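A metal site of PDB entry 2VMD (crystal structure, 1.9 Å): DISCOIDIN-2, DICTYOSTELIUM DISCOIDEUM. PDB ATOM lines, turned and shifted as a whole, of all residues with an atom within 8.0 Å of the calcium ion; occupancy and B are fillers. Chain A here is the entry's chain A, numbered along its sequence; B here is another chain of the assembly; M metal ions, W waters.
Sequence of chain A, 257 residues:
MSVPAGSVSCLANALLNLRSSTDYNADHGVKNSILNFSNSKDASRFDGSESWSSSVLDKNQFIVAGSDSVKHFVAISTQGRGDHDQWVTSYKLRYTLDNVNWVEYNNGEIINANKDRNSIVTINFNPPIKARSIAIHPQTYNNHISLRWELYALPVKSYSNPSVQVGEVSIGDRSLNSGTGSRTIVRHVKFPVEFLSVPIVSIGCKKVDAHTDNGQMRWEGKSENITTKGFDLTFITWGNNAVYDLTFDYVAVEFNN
N of Asp 42 lies close to OG of Ser 40 (3.4 Å).
The side-chain carboxylate of Asp 47 sits at hydrogen-bond distance from the side-chain hydroxyl of Ser 55 of chain B (2.6 Å).
The backbone carbonyl oxygen (O) of Asn 39 is in hydrogen-bond range of the side-chain amino group (NZ) of Lys 41.
The side-chain carboxylate (OE2) of Glu 50 is in hydrogen-bond range of the backbone NH (N) of Asn 39.
The side-chain amide nitrogen (ND2) of Asn 39 is in hydrogen-bond range of the backbone carbonyl oxygen (O) of Gly 48 (3.0 Å).
Of the 20 residues printed, 3 come within 4 Å of the calcium ion.
The nearest printed residue that does not touch the calcium ion is Gly 48 (4.4 Å).
O of Ser 40 is bound to the calcium ion.
The calcium ion is bound by water W1, 2.3 Å away.
The calcium ion is bound by water W2 (2.3 Å).
OD1 of Asn 39 binds the calcium ion.
The side-chain carboxylate (OD1) of Asp 47 is bound to the calcium ion, at 2.5 Å.
Water W3 is bound to the calcium ion.
The calcium ion is bound by water W4.
The calcium ion has seven donor atoms within binding distance.
Water W2 bridges O of Gly 48 (2.9 Å) and OD2 of Asp 83 (3.4 Å).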
ATOM      1  N   PHE A  37     -23.155 -21.031   2.306  1.00  0.00           N
ATOM      2  CA  PHE A  37     -23.543 -21.609   1.015  1.00  0.00           C
ATOM      3  C   PHE A  37     -22.322 -21.793   0.109  1.00  0.00           C
ATOM      4  O   PHE A  37     -21.482 -20.890  -0.036  1.00  0.00           O
ATOM      5  CB  PHE A  37     -24.580 -20.722   0.298  1.00  0.00           C
ATOM      6  CG  PHE A  37     -24.928 -21.178  -1.089  1.00  0.00           C
ATOM      7  CD1 PHE A  37     -25.875 -22.182  -1.282  1.00  0.00           C
ATOM      8  CD2 PHE A  37     -24.318 -20.612  -2.200  1.00  0.00           C
ATOM      9  CE1 PHE A  37     -26.189 -22.636  -2.561  1.00  0.00           C
ATOM     10  CE2 PHE A  37     -24.614 -21.065  -3.466  1.00  0.00           C
ATOM     11  CZ  PHE A  37     -25.557 -22.087  -3.646  1.00  0.00           C
ATOM     12  N   SER A  38     -22.224 -22.965  -0.501  1.00  0.00           N
ATOM     13  CA  SER A  38     -21.162 -23.177  -1.457  1.00  0.00           C
ATOM     14  C   SER A  38     -21.619 -24.163  -2.492  1.00  0.00           C
ATOM     15  O   SER A  38     -22.376 -25.061  -2.192  1.00  0.00           O
ATOM     16  CB  SER A  38     -19.882 -23.613  -0.751  1.00  0.00           C
ATOM     17  OG  SER A  38     -19.872 -25.003  -0.626  1.00  0.00           O
ATOM     18  N   ASN A  39     -21.176 -23.974  -3.727  1.00  0.00           N
ATOM     19  CA  ASN A  39     -21.639 -24.853  -4.781  1.00  0.00           C
ATOM     20  C   ASN A  39     -20.442 -25.475  -5.499  1.00  0.00           C
ATOM     21  O   ASN A  39     -19.410 -25.700  -4.860  1.00  0.00           O
ATOM     22  CB  ASN A  39     -22.665 -24.141  -5.689  1.00  0.00           C
ATOM     23  CG  ASN A  39     -22.162 -22.834  -6.260  1.00  0.00           C
ATOM     24  OD1 ASN A  39     -20.956 -22.628  -6.387  1.00  0.00           O
ATOM     25  ND2 ASN A  39     -23.089 -21.961  -6.684  1.00  0.00           N
ATOM     26  N   SER A  40     -20.560 -25.736  -6.784  1.00  0.00           N
ATOM     27  CA  SER A  40     -19.499 -26.444  -7.469  1.00  0.00           C
ATOM     28  C   SER A  40     -18.261 -25.583  -7.600  1.00  0.00           C
ATOM     29  O   SER A  40     -18.343 -24.427  -7.978  1.00  0.00           O
ATOM     30  CB  SER A  40     -19.954 -26.914  -8.833  1.00  0.00           C
ATOM     31  OG  SER A  40     -18.932 -27.673  -9.416  1.00  0.00           O
ATOM     32  N   LYS A  41     -17.103 -26.161  -7.307  1.00  0.00           N
ATOM     33  CA  LYS A  41     -15.836 -25.421  -7.380  1.00  0.00           C
ATOM     34  C   LYS A  41     -15.257 -25.430  -8.795  1.00  0.00           C
ATOM     35  O   LYS A  41     -14.125 -24.978  -9.024  1.00  0.00           O
ATOM     36  CB  LYS A  41     -14.838 -26.008  -6.383  1.00  0.00           C
ATOM     37  CG  LYS A  41     -15.237 -25.761  -4.956  1.00  0.00           C
ATOM     38  CD  LYS A  41     -15.450 -24.267  -4.737  1.00  0.00           C
ATOM     39  CE  LYS A  41     -15.757 -23.967  -3.291  1.00  0.00           C
ATOM     40  NZ  LYS A  41     -17.210 -24.069  -3.032  1.00  0.00           N
ATOM     41  N   ASP A  42     -16.035 -25.942  -9.729  1.00  0.00           N
ATOM     42  CA  ASP A  42     -15.716 -25.964 -11.153  1.00  0.00           C
ATOM     43  C   ASP A  42     -15.580 -24.566 -11.749  1.00  0.00           C
ATOM     44  O   ASP A  42     -16.541 -23.812 -11.818  1.00  0.00           O
ATOM     45  CB  ASP A  42     -16.820 -26.755 -11.885  1.00  0.00           C
ATOM     46  CG  ASP A  42     -16.590 -26.842 -13.377  1.00  0.00           C
ATOM     47  OD1 ASP A  42     -15.651 -26.177 -13.865  1.00  0.00           O
ATOM     48  OD2 ASP A  42     -17.340 -27.595 -14.056  1.00  0.00           O
ATOM     49  N   ALA A  43     -14.378 -24.227 -12.231  1.00  0.00           N
ATOM     50  CA  ALA A  43     -14.111 -22.893 -12.804  1.00  0.00           C
ATOM     51  C   ALA A  43     -14.624 -22.739 -14.237  1.00  0.00           C
ATOM     52  O   ALA A  43     -14.633 -21.635 -14.776  1.00  0.00           O
ATOM     53  CB  ALA A  43     -12.634 -22.585 -12.735  1.00  0.00           C
ATOM     54  N   SER A  44     -15.068 -23.824 -14.846  1.00  0.00           N
ATOM     55  CA  SER A  44     -15.443 -23.764 -16.254  1.00  0.00           C
ATOM     56  C   SER A  44     -16.924 -23.520 -16.506  1.00  0.00           C
ATOM     57  O   SER A  44     -17.319 -23.248 -17.653  1.00  0.00           O
ATOM     58  CB  SER A  44     -14.999 -25.048 -16.964  1.00  0.00           C
ATOM     59  OG  SER A  44     -15.952 -26.071 -16.786  1.00  0.00           O
ATOM     60  N   ARG A  45     -17.747 -23.620 -15.450  1.00  0.00           N
ATOM     61  CA  ARG A  45     -19.198 -23.444 -15.542  1.00  0.00           C
ATOM     62  C   ARG A  45     -19.688 -22.634 -14.347  1.00  0.00           C
ATOM     63  O   ARG A  45     -19.355 -22.952 -13.210  1.00  0.00           O
ATOM     64  CB  ARG A  45     -19.889 -24.802 -15.519  1.00  0.00           C
ATOM     65  CG  ARG A  45     -21.334 -24.803 -15.890  1.00  0.00           C
ATOM     66  CD  ARG A  45     -21.897 -26.207 -15.819  1.00  0.00           C
ATOM     67  NE  ARG A  45     -21.721 -26.850 -14.503  1.00  0.00           N
ATOM     68  CZ  ARG A  45     -22.481 -26.612 -13.435  1.00  0.00           C
ATOM     69  NH1 ARG A  45     -23.454 -25.711 -13.499  1.00  0.00           N
ATOM     70  NH2 ARG A  45     -22.273 -27.261 -12.292  1.00  0.00           N
ATOM     71  N   PHE A  46     -20.491 -21.614 -14.599  1.00  0.00           N
ATOM     72  CA  PHE A  46     -21.068 -20.837 -13.527  1.00  0.00           C
ATOM     73  C   PHE A  46     -22.399 -21.417 -13.082  1.00  0.00           C
ATOM     74  O   PHE A  46     -23.355 -21.446 -13.862  1.00  0.00           O
ATOM     75  CB  PHE A  46     -21.282 -19.426 -13.997  1.00  0.00           C
ATOM     76  CG  PHE A  46     -21.638 -18.484 -12.916  1.00  0.00           C
ATOM     77  CD1 PHE A  46     -20.848 -18.375 -11.780  1.00  0.00           C
ATOM     78  CD2 PHE A  46     -22.771 -17.692 -13.027  1.00  0.00           C
ATOM     79  CE1 PHE A  46     -21.175 -17.482 -10.768  1.00  0.00           C
ATOM     80  CE2 PHE A  46     -23.104 -16.795 -12.031  1.00  0.00           C
ATOM     81  CZ  PHE A  46     -22.302 -16.690 -10.887  1.00  0.00           C
ATOM     82  N   ASP A  47     -22.449 -21.882 -11.832  1.00  0.00           N
ATOM     83  CA  ASP A  47     -23.676 -22.380 -11.199  1.00  0.00           C
ATOM     84  C   ASP A  47     -24.349 -21.371 -10.244  1.00  0.00           C
ATOM     85  O   ASP A  47     -25.286 -21.726  -9.521  1.00  0.00           O
ATOM     86  CB  ASP A  47     -23.436 -23.721 -10.485  1.00  0.00           C
ATOM     87  CG  ASP A  47     -22.303 -23.671  -9.497  1.00  0.00           C
ATOM     88  OD1 ASP A  47     -21.586 -22.651  -9.400  1.00  0.00           O
ATOM     89  OD2 ASP A  47     -22.100 -24.670  -8.778  1.00  0.00           O
ATOM     90  N   GLY A  48     -23.874 -20.124 -10.256  1.00  0.00           N
ATOM     91  CA  GLY A  48     -24.437 -19.098  -9.407  1.00  0.00           C
ATOM     92  C   GLY A  48     -23.431 -18.574  -8.402  1.00  0.00           C
ATOM     93  O   GLY A  48     -22.501 -19.280  -8.010  1.00  0.00           O
ATOM     94  N   SER A  49     -23.622 -17.317  -7.982  1.00  0.00           N
ATOM     95  CA  SER A  49     -22.752 -16.767  -6.958  1.00  0.00           C
ATOM     96  C   SER A  49     -22.958 -17.497  -5.609  1.00  0.00           C
ATOM     97  O   SER A  49     -24.076 -17.927  -5.284  1.00  0.00           O
ATOM     98  CB  SER A  49     -23.099 -15.299  -6.785  1.00  0.00           C
ATOM     99  OG  SER A  49     -24.472 -15.153  -6.413  1.00  0.00           O
ATOM    100  N   GLU A  50     -21.907 -17.580  -4.786  1.00  0.00           N
ATOM    101  CA  GLU A  50     -22.072 -18.033  -3.395  1.00  0.00           C
ATOM    102  C   GLU A  50     -22.463 -16.819  -2.532  1.00  0.00           C
ATOM    103  O   GLU A  50     -21.727 -16.378  -1.647  1.00  0.00           O
ATOM    104  CB  GLU A  50     -20.794 -18.779  -2.925  1.00  0.00           C
ATOM    105  CG  GLU A  50     -20.486 -20.031  -3.812  1.00  0.00           C
ATOM    106  CD  GLU A  50     -19.186 -20.759  -3.447  1.00  0.00           C
ATOM    107  OE1 GLU A  50     -18.342 -20.130  -2.811  1.00  0.00           O
ATOM    108  OE2 GLU A  50     -19.022 -21.984  -3.785  1.00  0.00           O
ATOM    109  N   ARG A  81     -19.250 -12.927   0.011  1.00  0.00           N
ATOM    110  CA  ARG A  81     -19.436 -13.854  -1.076  1.00  0.00           C
ATOM    111  C   ARG A  81     -18.331 -14.955  -1.110  1.00  0.00           C
ATOM    112  O   ARG A  81     -17.150 -14.682  -0.980  1.00  0.00           O
ATOM    113  CB  ARG A  81     -19.577 -13.068  -2.404  1.00  0.00           C
ATOM    114  CG  ARG A  81     -19.557 -13.964  -3.602  1.00  0.00           C
ATOM    115  CD  ARG A  81     -19.906 -13.219  -4.844  1.00  0.00           C
ATOM    116  NE  ARG A  81     -19.837 -14.111  -5.996  1.00  0.00           N
ATOM    117  CZ  ARG A  81     -20.007 -13.729  -7.258  1.00  0.00           C
ATOM    118  NH1 ARG A  81     -20.313 -12.463  -7.524  1.00  0.00           N
ATOM    119  NH2 ARG A  81     -19.919 -14.620  -8.226  1.00  0.00           N
ATOM    120  N   ASP A  83     -17.325 -17.037  -3.623  1.00  0.00           N
ATOM    121  CA  ASP A  83     -16.576 -17.304  -4.860  1.00  0.00           C
ATOM    122  C   ASP A  83     -15.955 -16.099  -5.566  1.00  0.00           C
ATOM    123  O   ASP A  83     -15.308 -16.250  -6.607  1.00  0.00           O
ATOM    124  CB  ASP A  83     -17.448 -18.080  -5.856  1.00  0.00           C
ATOM    125  CG  ASP A  83     -18.664 -17.289  -6.279  1.00  0.00           C
ATOM    126  OD1 ASP A  83     -19.330 -16.723  -5.384  1.00  0.00           O
ATOM    127  OD2 ASP A  83     -18.910 -17.204  -7.499  1.00  0.00           O
ATOM    128  N   ASP B  23     -27.873 -25.743  -6.841  1.00  0.00           N
ATOM    129  CA  ASP B  23     -28.649 -25.812  -8.073  1.00  0.00           C
ATOM    130  C   ASP B  23     -27.638 -25.795  -9.202  1.00  0.00           C
ATOM    131  O   ASP B  23     -26.680 -25.043  -9.146  1.00  0.00           O
ATOM    132  CB  ASP B  23     -29.517 -24.560  -8.289  1.00  0.00           C
ATOM    133  CG  ASP B  23     -30.630 -24.422  -7.290  1.00  0.00           C
ATOM    134  OD1 ASP B  23     -31.075 -25.450  -6.702  1.00  0.00           O
ATOM    135  OD2 ASP B  23     -31.077 -23.265  -7.127  1.00  0.00           O
ATOM    136  N   TYR B  24     -27.897 -26.568 -10.265  1.00  0.00           N
ATOM    137  CA  TYR B  24     -27.058 -26.513 -11.472  1.00  0.00           C
ATOM    138  C   TYR B  24     -26.890 -25.092 -11.958  1.00  0.00           C
ATOM    139  O   TYR B  24     -25.780 -24.645 -12.251  1.00  0.00           O
ATOM    140  CB  TYR B  24     -27.617 -27.391 -12.554  1.00  0.00           C
ATOM    141  CG  TYR B  24     -26.628 -27.692 -13.654  1.00  0.00           C
ATOM    142  CD1 TYR B  24     -25.633 -28.665 -13.472  1.00  0.00           C
ATOM    143  CD2 TYR B  24     -26.702 -27.028 -14.874  1.00  0.00           C
ATOM    144  CE1 TYR B  24     -24.729 -28.967 -14.497  1.00  0.00           C
ATOM    145  CE2 TYR B  24     -25.802 -27.312 -15.911  1.00  0.00           C
ATOM    146  CZ  TYR B  24     -24.830 -28.288 -15.697  1.00  0.00           C
ATOM    147  OH  TYR B  24     -23.959 -28.580 -16.706  1.00  0.00           O
ATOM    148  N   SER B  55     -26.121 -28.929  -8.406  1.00  0.00           N
ATOM    149  CA  SER B  55     -24.875 -28.585  -9.126  1.00  0.00           C
ATOM    150  C   SER B  55     -23.804 -29.604  -8.750  1.00  0.00           C
ATOM    151  O   SER B  55     -23.141 -30.163  -9.609  1.00  0.00           O
ATOM    152  CB  SER B  55     -24.355 -27.204  -8.730  1.00  0.00           C
ATOM    153  OG  SER B  55     -23.199 -26.890  -9.513  1.00  0.00           O
ATOM    154  N   VAL B  56     -23.640 -29.852  -7.455  1.00  0.00           N
ATOM    155  CA  VAL B  56     -22.660 -30.833  -7.017  1.00  0.00           C
ATOM    156  C   VAL B  56     -23.284 -32.212  -7.119  1.00  0.00           C
ATOM    157  O   VAL B  56     -24.464 -32.394  -6.741  1.00  0.00           O
ATOM    158  CB  VAL B  56     -22.168 -30.477  -5.589  1.00  0.00           C
ATOM    159  CG1 VAL B  56     -21.205 -31.571  -4.978  1.00  0.00           C
ATOM    160  CG2 VAL B  56     -21.464 -29.128  -5.581  1.00  0.00           C
HETATM  161 CA    CA M   1     -19.372 -22.390  -8.282  1.00  0.00          CA
HETATM  162  O   HOH W   1     -18.207 -21.569  -6.447  1.00  0.00           O
HETATM  163  O   HOH W   2     -19.915 -20.182  -8.857  1.00  0.00           O
HETATM  164  O   HOH W   3     -17.123 -21.607  -9.161  1.00  0.00           O
HETATM  165  O   HOH W   4     -18.859 -23.202 -10.813  1.00  0.00           O
